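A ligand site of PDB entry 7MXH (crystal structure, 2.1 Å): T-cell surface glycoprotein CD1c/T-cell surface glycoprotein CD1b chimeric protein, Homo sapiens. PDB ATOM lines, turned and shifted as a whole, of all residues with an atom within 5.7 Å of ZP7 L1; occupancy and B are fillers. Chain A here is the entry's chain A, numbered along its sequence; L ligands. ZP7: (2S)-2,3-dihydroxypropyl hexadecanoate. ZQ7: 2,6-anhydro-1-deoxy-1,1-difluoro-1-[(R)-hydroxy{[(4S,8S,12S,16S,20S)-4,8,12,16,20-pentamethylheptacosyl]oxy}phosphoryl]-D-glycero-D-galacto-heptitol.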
ATOM      1  N   PHE A  72     -18.102  12.736  12.613  1.00  0.00           N
ATOM      2  CA  PHE A  72     -18.918  13.854  12.173  1.00  0.00           C
ATOM      3  C   PHE A  72     -19.583  13.553  10.840  1.00  0.00           C
ATOM      4  O   PHE A  72     -20.787  13.774  10.665  1.00  0.00           O
ATOM      5  CB  PHE A  72     -18.054  15.119  12.054  1.00  0.00           C
ATOM      6  CG  PHE A  72     -17.984  15.922  13.315  1.00  0.00           C
ATOM      7  CD1 PHE A  72     -19.135  16.377  13.945  1.00  0.00           C
ATOM      8  CD2 PHE A  72     -16.749  16.243  13.881  1.00  0.00           C
ATOM      9  CE1 PHE A  72     -19.062  17.119  15.114  1.00  0.00           C
ATOM     10  CE2 PHE A  72     -16.675  16.985  15.050  1.00  0.00           C
ATOM     11  CZ  PHE A  72     -17.827  17.417  15.671  1.00  0.00           C
ATOM     12  N   TYR A  73     -18.813  13.040   9.897  1.00  0.00           N
ATOM     13  CA  TYR A  73     -19.335  12.723   8.577  1.00  0.00           C
ATOM     14  C   TYR A  73     -20.431  11.671   8.645  1.00  0.00           C
ATOM     15  O   TYR A  73     -21.476  11.802   8.013  1.00  0.00           O
ATOM     16  CB  TYR A  73     -18.176  12.239   7.702  1.00  0.00           C
ATOM     17  CG  TYR A  73     -18.528  11.289   6.578  1.00  0.00           C
ATOM     18  CD1 TYR A  73     -19.092  11.762   5.408  1.00  0.00           C
ATOM     19  CD2 TYR A  73     -18.235   9.934   6.664  1.00  0.00           C
ATOM     20  CE1 TYR A  73     -19.387  10.914   4.351  1.00  0.00           C
ATOM     21  CE2 TYR A  73     -18.531   9.068   5.620  1.00  0.00           C
ATOM     22  CZ  TYR A  73     -19.102   9.576   4.460  1.00  0.00           C
ATOM     23  OH  TYR A  73     -19.396   8.755   3.379  1.00  0.00           O
ATOM     24  N   PHE A  75     -22.360  10.590  11.310  1.00  0.00           N
ATOM     25  CA  PHE A  75     -23.555  11.081  12.006  1.00  0.00           C
ATOM     26  C   PHE A  75     -24.321  12.073  11.153  1.00  0.00           C
ATOM     27  O   PHE A  75     -25.554  12.021  11.108  1.00  0.00           O
ATOM     28  CB  PHE A  75     -23.178  11.737  13.338  1.00  0.00           C
ATOM     29  CG  PHE A  75     -22.523  10.811  14.322  1.00  0.00           C
ATOM     30  CD1 PHE A  75     -22.502   9.435  14.115  1.00  0.00           C
ATOM     31  CD2 PHE A  75     -21.892  11.337  15.456  1.00  0.00           C
ATOM     32  CE1 PHE A  75     -21.885   8.592  15.032  1.00  0.00           C
ATOM     33  CE2 PHE A  75     -21.272  10.503  16.370  1.00  0.00           C
ATOM     34  CZ  PHE A  75     -21.267   9.119  16.158  1.00  0.00           C
ATOM     35  N   GLY A  76     -23.609  12.991  10.479  1.00  0.00           N
ATOM     36  CA  GLY A  76     -24.295  13.965   9.651  1.00  0.00           C
ATOM     37  C   GLY A  76     -24.949  13.334   8.428  1.00  0.00           C
ATOM     38  O   GLY A  76     -26.064  13.714   8.057  1.00  0.00           O
ATOM     39  N   LEU A  77     -24.272  12.378   7.793  1.00  0.00           N
ATOM     40  CA  LEU A  77     -24.848  11.648   6.669  1.00  0.00           C
ATOM     41  C   LEU A  77     -26.137  10.950   7.087  1.00  0.00           C
ATOM     42  O   LEU A  77     -27.175  11.073   6.421  1.00  0.00           O
ATOM     43  CB  LEU A  77     -23.836  10.637   6.129  1.00  0.00           C
ATOM     44  CG  LEU A  77     -24.229   9.880   4.854  1.00  0.00           C
ATOM     45  CD1 LEU A  77     -24.709  10.832   3.771  1.00  0.00           C
ATOM     46  CD2 LEU A  77     -23.067   9.030   4.330  1.00  0.00           C
ATOM     47  N   ARG A  79     -28.093  11.511   9.735  1.00  0.00           N
ATOM     48  CA  ARG A  79     -29.119  12.479  10.080  1.00  0.00           C
ATOM     49  C   ARG A  79     -29.771  13.081   8.845  1.00  0.00           C
ATOM     50  O   ARG A  79     -31.001  13.132   8.737  1.00  0.00           O
ATOM     51  CB  ARG A  79     -28.489  13.569  10.961  1.00  0.00           C
ATOM     52  CG  ARG A  79     -29.477  14.457  11.663  1.00  0.00           C
ATOM     53  CD  ARG A  79     -28.779  15.732  12.064  1.00  0.00           C
ATOM     54  NE  ARG A  79     -27.474  15.425  12.659  1.00  0.00           N
ATOM     55  CZ  ARG A  79     -26.335  16.009  12.306  1.00  0.00           C
ATOM     56  NH1 ARG A  79     -25.203  15.647  12.905  1.00  0.00           N
ATOM     57  NH2 ARG A  79     -26.322  16.934  11.364  1.00  0.00           N
ATOM     58  N   GLU A  80     -28.969  13.516   7.881  1.00  0.00           N
ATOM     59  CA  GLU A  80     -29.500  14.167   6.693  1.00  0.00           C
ATOM     60  C   GLU A  80     -30.360  13.217   5.875  1.00  0.00           C
ATOM     61  O   GLU A  80     -31.494  13.566   5.480  1.00  0.00           O
ATOM     62  CB  GLU A  80     -28.353  14.707   5.850  1.00  0.00           C
ATOM     63  CG  GLU A  80     -27.662  15.891   6.486  1.00  0.00           C
ATOM     64  CD  GLU A  80     -28.678  16.875   7.041  1.00  0.00           C
ATOM     65  OE1 GLU A  80     -28.784  16.954   8.291  1.00  0.00           O
ATOM     66  OE2 GLU A  80     -29.376  17.526   6.214  1.00  0.00           O
ATOM     67  N   ILE A  81     -29.855  12.010   5.613  1.00  0.00           N
ATOM     68  CA  ILE A  81     -30.601  11.035   4.830  1.00  0.00           C
ATOM     69  C   ILE A  81     -31.922  10.702   5.505  1.00  0.00           C
ATOM     70  O   ILE A  81     -32.984  10.689   4.870  1.00  0.00           O
ATOM     71  CB  ILE A  81     -29.748   9.770   4.606  1.00  0.00           C
ATOM     72  CG1 ILE A  81     -28.566  10.074   3.684  1.00  0.00           C
ATOM     73  CG2 ILE A  81     -30.595   8.643   4.043  1.00  0.00           C
ATOM     74  CD1 ILE A  81     -27.784   8.855   3.269  1.00  0.00           C
ATOM     75  N   HIS A  84     -34.476  13.414   5.158  1.00  0.00           N
ATOM     76  CA  HIS A  84     -35.070  13.625   3.840  1.00  0.00           C
ATOM     77  C   HIS A  84     -36.016  12.499   3.410  1.00  0.00           C
ATOM     78  O   HIS A  84     -36.878  12.727   2.563  1.00  0.00           O
ATOM     79  CB  HIS A  84     -33.969  13.835   2.807  1.00  0.00           C
ATOM     80  CG  HIS A  84     -33.307  15.168   2.906  1.00  0.00           C
ATOM     81  ND1 HIS A  84     -33.792  16.304   2.279  1.00  0.00           N
ATOM     82  CD2 HIS A  84     -32.211  15.573   3.600  1.00  0.00           C
ATOM     83  CE1 HIS A  84     -33.017  17.335   2.566  1.00  0.00           C
ATOM     84  NE2 HIS A  84     -32.046  16.919   3.368  1.00  0.00           N
ATOM     85  N   SER A 139     -33.085  11.057 -11.675  1.00  0.00           N
ATOM     86  CA  SER A 139     -33.592  12.198 -10.926  1.00  0.00           C
ATOM     87  C   SER A 139     -33.072  12.233  -9.484  1.00  0.00           C
ATOM     88  O   SER A 139     -32.718  13.290  -8.959  1.00  0.00           O
ATOM     89  CB  SER A 139     -35.126  12.151 -10.945  1.00  0.00           C
ATOM     90  OG  SER A 139     -35.657  12.934  -9.900  1.00  0.00           O
ATOM     91  N   LEU A 140     -33.017  11.062  -8.845  1.00  0.00           N
ATOM     92  CA  LEU A 140     -32.495  11.017  -7.483  1.00  0.00           C
ATOM     93  C   LEU A 140     -31.050  11.477  -7.425  1.00  0.00           C
ATOM     94  O   LEU A 140     -30.670  12.241  -6.520  1.00  0.00           O
ATOM     95  CB  LEU A 140     -32.637   9.603  -6.911  1.00  0.00           C
ATOM     96  CG  LEU A 140     -32.020   9.452  -5.521  1.00  0.00           C
ATOM     97  CD1 LEU A 140     -32.833  10.238  -4.490  1.00  0.00           C
ATOM     98  CD2 LEU A 140     -31.886   7.971  -5.120  1.00  0.00           C
ATOM     99  N   SER A 143     -30.861  15.232  -7.621  1.00  0.00           N
ATOM    100  CA  SER A 143     -31.300  15.917  -6.398  1.00  0.00           C
ATOM    101  C   SER A 143     -30.245  15.832  -5.292  1.00  0.00           C
ATOM    102  O   SER A 143     -29.957  16.824  -4.598  1.00  0.00           O
ATOM    103  CB  SER A 143     -32.616  15.325  -5.904  1.00  0.00           C
ATOM    104  OG  SER A 143     -33.637  15.392  -6.892  1.00  0.00           O
ATOM    105  N   VAL A 144     -29.660  14.655  -5.115  1.00  0.00           N
ATOM    106  CA  VAL A 144     -28.609  14.530  -4.111  1.00  0.00           C
ATOM    107  C   VAL A 144     -27.453  15.471  -4.448  1.00  0.00           C
ATOM    108  O   VAL A 144     -26.897  16.159  -3.569  1.00  0.00           O
ATOM    109  CB  VAL A 144     -28.154  13.063  -3.989  1.00  0.00           C
ATOM    110  CG1 VAL A 144     -27.084  12.893  -2.914  1.00  0.00           C
ATOM    111  CG2 VAL A 144     -29.355  12.173  -3.672  1.00  0.00           C
ATOM    112  N   LEU A 147     -28.049  19.106  -3.555  1.00  0.00           N
ATOM    113  CA  LEU A 147     -27.842  19.414  -2.139  1.00  0.00           C
ATOM    114  C   LEU A 147     -26.365  19.456  -1.788  1.00  0.00           C
ATOM    115  O   LEU A 147     -25.913  20.354  -1.071  1.00  0.00           O
ATOM    116  CB  LEU A 147     -28.581  18.407  -1.255  1.00  0.00           C
ATOM    117  CG  LEU A 147     -30.103  18.460  -1.342  1.00  0.00           C
ATOM    118  CD1 LEU A 147     -30.684  17.347  -0.506  1.00  0.00           C
ATOM    119  CD2 LEU A 147     -30.638  19.833  -0.913  1.00  0.00           C
ATOM    120  N   LEU A 148     -25.588  18.489  -2.278  1.00  0.00           N
ATOM    121  CA  LEU A 148     -24.173  18.426  -1.905  1.00  0.00           C
ATOM    122  C   LEU A 148     -23.406  19.628  -2.443  1.00  0.00           C
ATOM    123  O   LEU A 148     -22.537  20.181  -1.753  1.00  0.00           O
ATOM    124  CB  LEU A 148     -23.562  17.113  -2.400  1.00  0.00           C
ATOM    125  CG  LEU A 148     -24.068  15.826  -1.758  1.00  0.00           C
ATOM    126  CD1 LEU A 148     -23.573  14.618  -2.539  1.00  0.00           C
ATOM    127  CD2 LEU A 148     -23.646  15.745  -0.292  1.00  0.00           C
ATOM    128  N   TYR A 152     -24.027  21.777   1.413  1.00  0.00           N
ATOM    129  CA  TYR A 152     -22.791  21.403   2.103  1.00  0.00           C
ATOM    130  C   TYR A 152     -21.560  21.777   1.286  1.00  0.00           C
ATOM    131  O   TYR A 152     -20.561  21.049   1.272  1.00  0.00           O
ATOM    132  CB  TYR A 152     -22.809  19.916   2.422  1.00  0.00           C
ATOM    133  CG  TYR A 152     -24.131  19.503   3.009  1.00  0.00           C
ATOM    134  CD1 TYR A 152     -24.369  19.559   4.386  1.00  0.00           C
ATOM    135  CD2 TYR A 152     -25.169  19.068   2.189  1.00  0.00           C
ATOM    136  CE1 TYR A 152     -25.596  19.192   4.912  1.00  0.00           C
ATOM    137  CE2 TYR A 152     -26.390  18.697   2.703  1.00  0.00           C
ATOM    138  CZ  TYR A 152     -26.605  18.765   4.070  1.00  0.00           C
ATOM    139  OH  TYR A 152     -27.846  18.395   4.559  1.00  0.00           O
ATOM    140  N   VAL A 155     -17.749  21.666   2.556  1.00  0.00           N
ATOM    141  CA  VAL A 155     -17.014  20.440   2.864  1.00  0.00           C
ATOM    142  C   VAL A 155     -16.411  19.791   1.631  1.00  0.00           C
ATOM    143  O   VAL A 155     -15.563  18.893   1.772  1.00  0.00           O
ATOM    144  CB  VAL A 155     -17.890  19.408   3.630  1.00  0.00           C
ATOM    145  CG1 VAL A 155     -18.606  20.063   4.787  1.00  0.00           C
ATOM    146  CG2 VAL A 155     -18.854  18.705   2.678  1.00  0.00           C
HETATM  147  C01 ZP7 L   1     -21.067  17.500  10.622  1.00  0.00           C
HETATM  148  C02 ZP7 L   1     -21.272  17.208   9.130  1.00  0.00           C
HETATM  149  C03 ZP7 L   1     -22.705  17.506   8.690  1.00  0.00           C
HETATM  150  C04 ZP7 L   1     -23.184  16.656   7.519  1.00  0.00           C
HETATM  151  C05 ZP7 L   1     -22.259  15.490   7.143  1.00  0.00           C
HETATM  152  C06 ZP7 L   1     -22.099  15.399   5.638  1.00  0.00           C
HETATM  153  C07 ZP7 L   1     -23.157  14.534   4.970  1.00  0.00           C
HETATM  154  C08 ZP7 L   1     -24.029  15.333   4.001  1.00  0.00           C
HETATM  155  C09 ZP7 L   1     -24.745  14.434   2.997  1.00  0.00           C
HETATM  156  C10 ZP7 L   1     -26.148  14.918   2.690  1.00  0.00           C
HETATM  157  C11 ZP7 L   1     -26.954  13.856   1.914  1.00  0.00           C
HETATM  158  C12 ZP7 L   1     -28.439  14.206   1.895  1.00  0.00           C
HETATM  159  C13 ZP7 L   1     -29.243  13.313   0.955  1.00  0.00           C
HETATM  160  C14 ZP7 L   1     -30.554  13.981   0.533  1.00  0.00           C
HETATM  161  C15 ZP7 L   1     -31.443  13.066  -0.310  1.00  0.00           C
HETATM  162  C16 ZP7 L   1     -32.626  13.847  -0.895  1.00  0.00           C
HETATM  163  C19 ZP7 L   1     -33.928  14.196  -2.810  1.00  0.00           C
HETATM  164  C20 ZP7 L   1     -35.305  13.766  -3.324  1.00  0.00           C
HETATM  165  C21 ZP7 L   1     -35.246  13.212  -4.751  1.00  0.00           C
HETATM  166  O17 ZP7 L   1     -32.815  14.964  -0.528  1.00  0.00           O
HETATM  167  O18 ZP7 L   1     -33.476  13.281  -1.848  1.00  0.00           O
HETATM  168  O22 ZP7 L   1     -36.193  13.877  -5.541  1.00  0.00           O
HETATM  169  O23 ZP7 L   1     -36.146  14.906  -3.297  1.00  0.00           O
HETATM  170  C1  ZQ7 L   2     -15.632  19.349  10.780  1.00  0.00           C
HETATM  171  C10 ZQ7 L   2     -13.388  10.300   3.011  1.00  0.00           C
HETATM  172  C11 ZQ7 L   2      -7.455   6.653   7.746  1.00  0.00           C
HETATM  173  C12 ZQ7 L   2     -15.289  11.230   4.355  1.00  0.00           C
HETATM  174  C13 ZQ7 L   2      -7.695   5.143   7.561  1.00  0.00           C
HETATM  175  C14 ZQ7 L   2      -8.579   4.575   8.652  1.00  0.00           C
HETATM  176  C15 ZQ7 L   2      -9.944   4.232   8.051  1.00  0.00           C
HETATM  177  C16 ZQ7 L   2     -15.189  12.332   5.462  1.00  0.00           C
HETATM  178  C17 ZQ7 L   2     -15.328  13.720   4.781  1.00  0.00           C
HETATM  179  C18 ZQ7 L   2     -16.459  14.519   5.415  1.00  0.00           C
HETATM  180  C19 ZQ7 L   2      -9.622   8.038   1.974  1.00  0.00           C
HETATM  181  C2  ZQ7 L   2      -9.807   8.719   3.329  1.00  0.00           C
HETATM  182  C20 ZQ7 L   2     -10.722   3.380   9.022  1.00  0.00           C
HETATM  183  C21 ZQ7 L   2      -5.792   8.235   6.706  1.00  0.00           C
HETATM  184  C22 ZQ7 L   2     -14.531   8.918   4.761  1.00  0.00           C
HETATM  185  C23 ZQ7 L   2     -15.850  15.763   6.076  1.00  0.00           C
HETATM  186  C24 ZQ7 L   2     -12.053   2.960   8.404  1.00  0.00           C
HETATM  187  C25 ZQ7 L   2      -9.708   3.399   6.808  1.00  0.00           C
HETATM  188  C26 ZQ7 L   2     -17.143  21.308  13.773  1.00  0.00           C
HETATM  189  C27 ZQ7 L   2     -16.078  20.656  14.636  1.00  0.00           C
HETATM  190  C28 ZQ7 L   2     -17.177  20.573  12.417  1.00  0.00           C
HETATM  191  C29 ZQ7 L   2     -14.731  20.931  13.967  1.00  0.00           C
HETATM  192  C3  ZQ7 L   2      -6.961   7.276   6.430  1.00  0.00           C
HETATM  193  C30 ZQ7 L   2     -17.452  14.942   4.343  1.00  0.00           C
HETATM  194  C31 ZQ7 L   2     -15.769  20.527  11.765  1.00  0.00           C
HETATM  195  C32 ZQ7 L   2     -16.519  16.050   7.420  1.00  0.00           C
HETATM  196  C33 ZQ7 L   2     -13.018   4.142   8.580  1.00  0.00           C
HETATM  197  C34 ZQ7 L   2     -14.377   3.765   8.033  1.00  0.00           C
HETATM  198  C35 ZQ7 L   2     -16.822  17.559   7.409  1.00  0.00           C
HETATM  199  C36 ZQ7 L   2     -13.610  20.278  14.798  1.00  0.00           C
HETATM  200  C37 ZQ7 L   2     -14.992   5.011   7.402  1.00  0.00           C
HETATM  201  C38 ZQ7 L   2     -16.143   5.523   8.272  1.00  0.00           C
HETATM  202  C39 ZQ7 L   2     -17.210   4.436   8.364  1.00  0.00           C
HETATM  203  C4  ZQ7 L   2      -8.539   9.538   3.678  1.00  0.00           C
HETATM  204  C5  ZQ7 L   2     -10.922   9.783   3.112  1.00  0.00           C
HETATM  205  C6  ZQ7 L   2     -14.059  10.311   4.401  1.00  0.00           C
HETATM  206  C7  ZQ7 L   2      -8.072   8.134   5.747  1.00  0.00           C
HETATM  207  C8  ZQ7 L   2      -7.461   8.741   4.464  1.00  0.00           C
HETATM  208  C9  ZQ7 L   2     -12.337   9.135   2.941  1.00  0.00           C
HETATM  209  F1  ZQ7 L   2     -14.318  19.290  10.420  1.00  0.00           F
HETATM  210  F2  ZQ7 L   2     -15.954  18.192  11.439  1.00  0.00           F
HETATM  211  O1  ZQ7 L   2     -14.699  20.389  12.676  1.00  0.00           O
HETATM  212  O2  ZQ7 L   2     -18.391  21.230  14.399  1.00  0.00           O
HETATM  213  O3  ZQ7 L   2     -16.103  21.176  15.936  1.00  0.00           O
HETATM  214  O4  ZQ7 L   2     -17.653  19.288  12.620  1.00  0.00           O
HETATM  215  O5  ZQ7 L   2     -17.170  17.972   8.720  1.00  0.00           O
HETATM  216  O6  ZQ7 L   2     -13.039  21.195  15.684  1.00  0.00           O
HETATM  217  O7  ZQ7 L   2     -17.726  20.434   9.285  1.00  0.00           O
HETATM  218  O8  ZQ7 L   2     -15.845  20.058   8.103  1.00  0.00           O
HETATM  219  P1  ZQ7 L   2     -16.623  19.481   9.188  1.00  0.00           P
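The backbone carbonyl oxygen (O) of Leu 147 sits at hydrogen-bond distance from the backbone NH (N) of Tyr 152 (3.4 Å). OH of Tyr 152 sits at hydrogen-bond distance from OE2 of Glu 80. OG of Ser 143 lies within hydrogen-bond range of O of Ser 139, at 3.1 Å. The guanidinium group (NH2) of Arg 79 lies within salt-bridge range of the side-chain carboxylate (OE1) of Glu 80 (3.9 Å).
Merely in contact with ZP7 L1: Phe 72 (3.7 Å), Tyr 73 (3.9 Å), Gly 76 (3.6 Å), Leu 77 (3.7 Å), Glu 80 (3.9 Å), Leu 140 (3.8 Å), Leu 147 (3.2 Å), Leu 148 (3.7 Å) and Tyr 152 (3.8 Å). Hydrophobic or aromatic side chains that line ZP7 L1: Leu 77, His 84, Leu 140, Leu 147, Leu 148 and Tyr 152. Within 4 Å of ZP7 L1: Phe 72, Tyr 73, Gly 76, Leu 77, Glu 80, His 84, Leu 140, Ser 143, Leu 147, Leu 148 and Tyr 152. The nearest printed residue that does not touch ZP7 L1 is Val 144 (4.1 Å).
OG of Ser 143 sits at hydrogen-bond distance from O22 of ZP7 L1 (3.3 Å). An oxygen (O17) of ZP7 L1 sits at hydrogen-bond distance from a ring nitrogen (ND1) of His 84.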
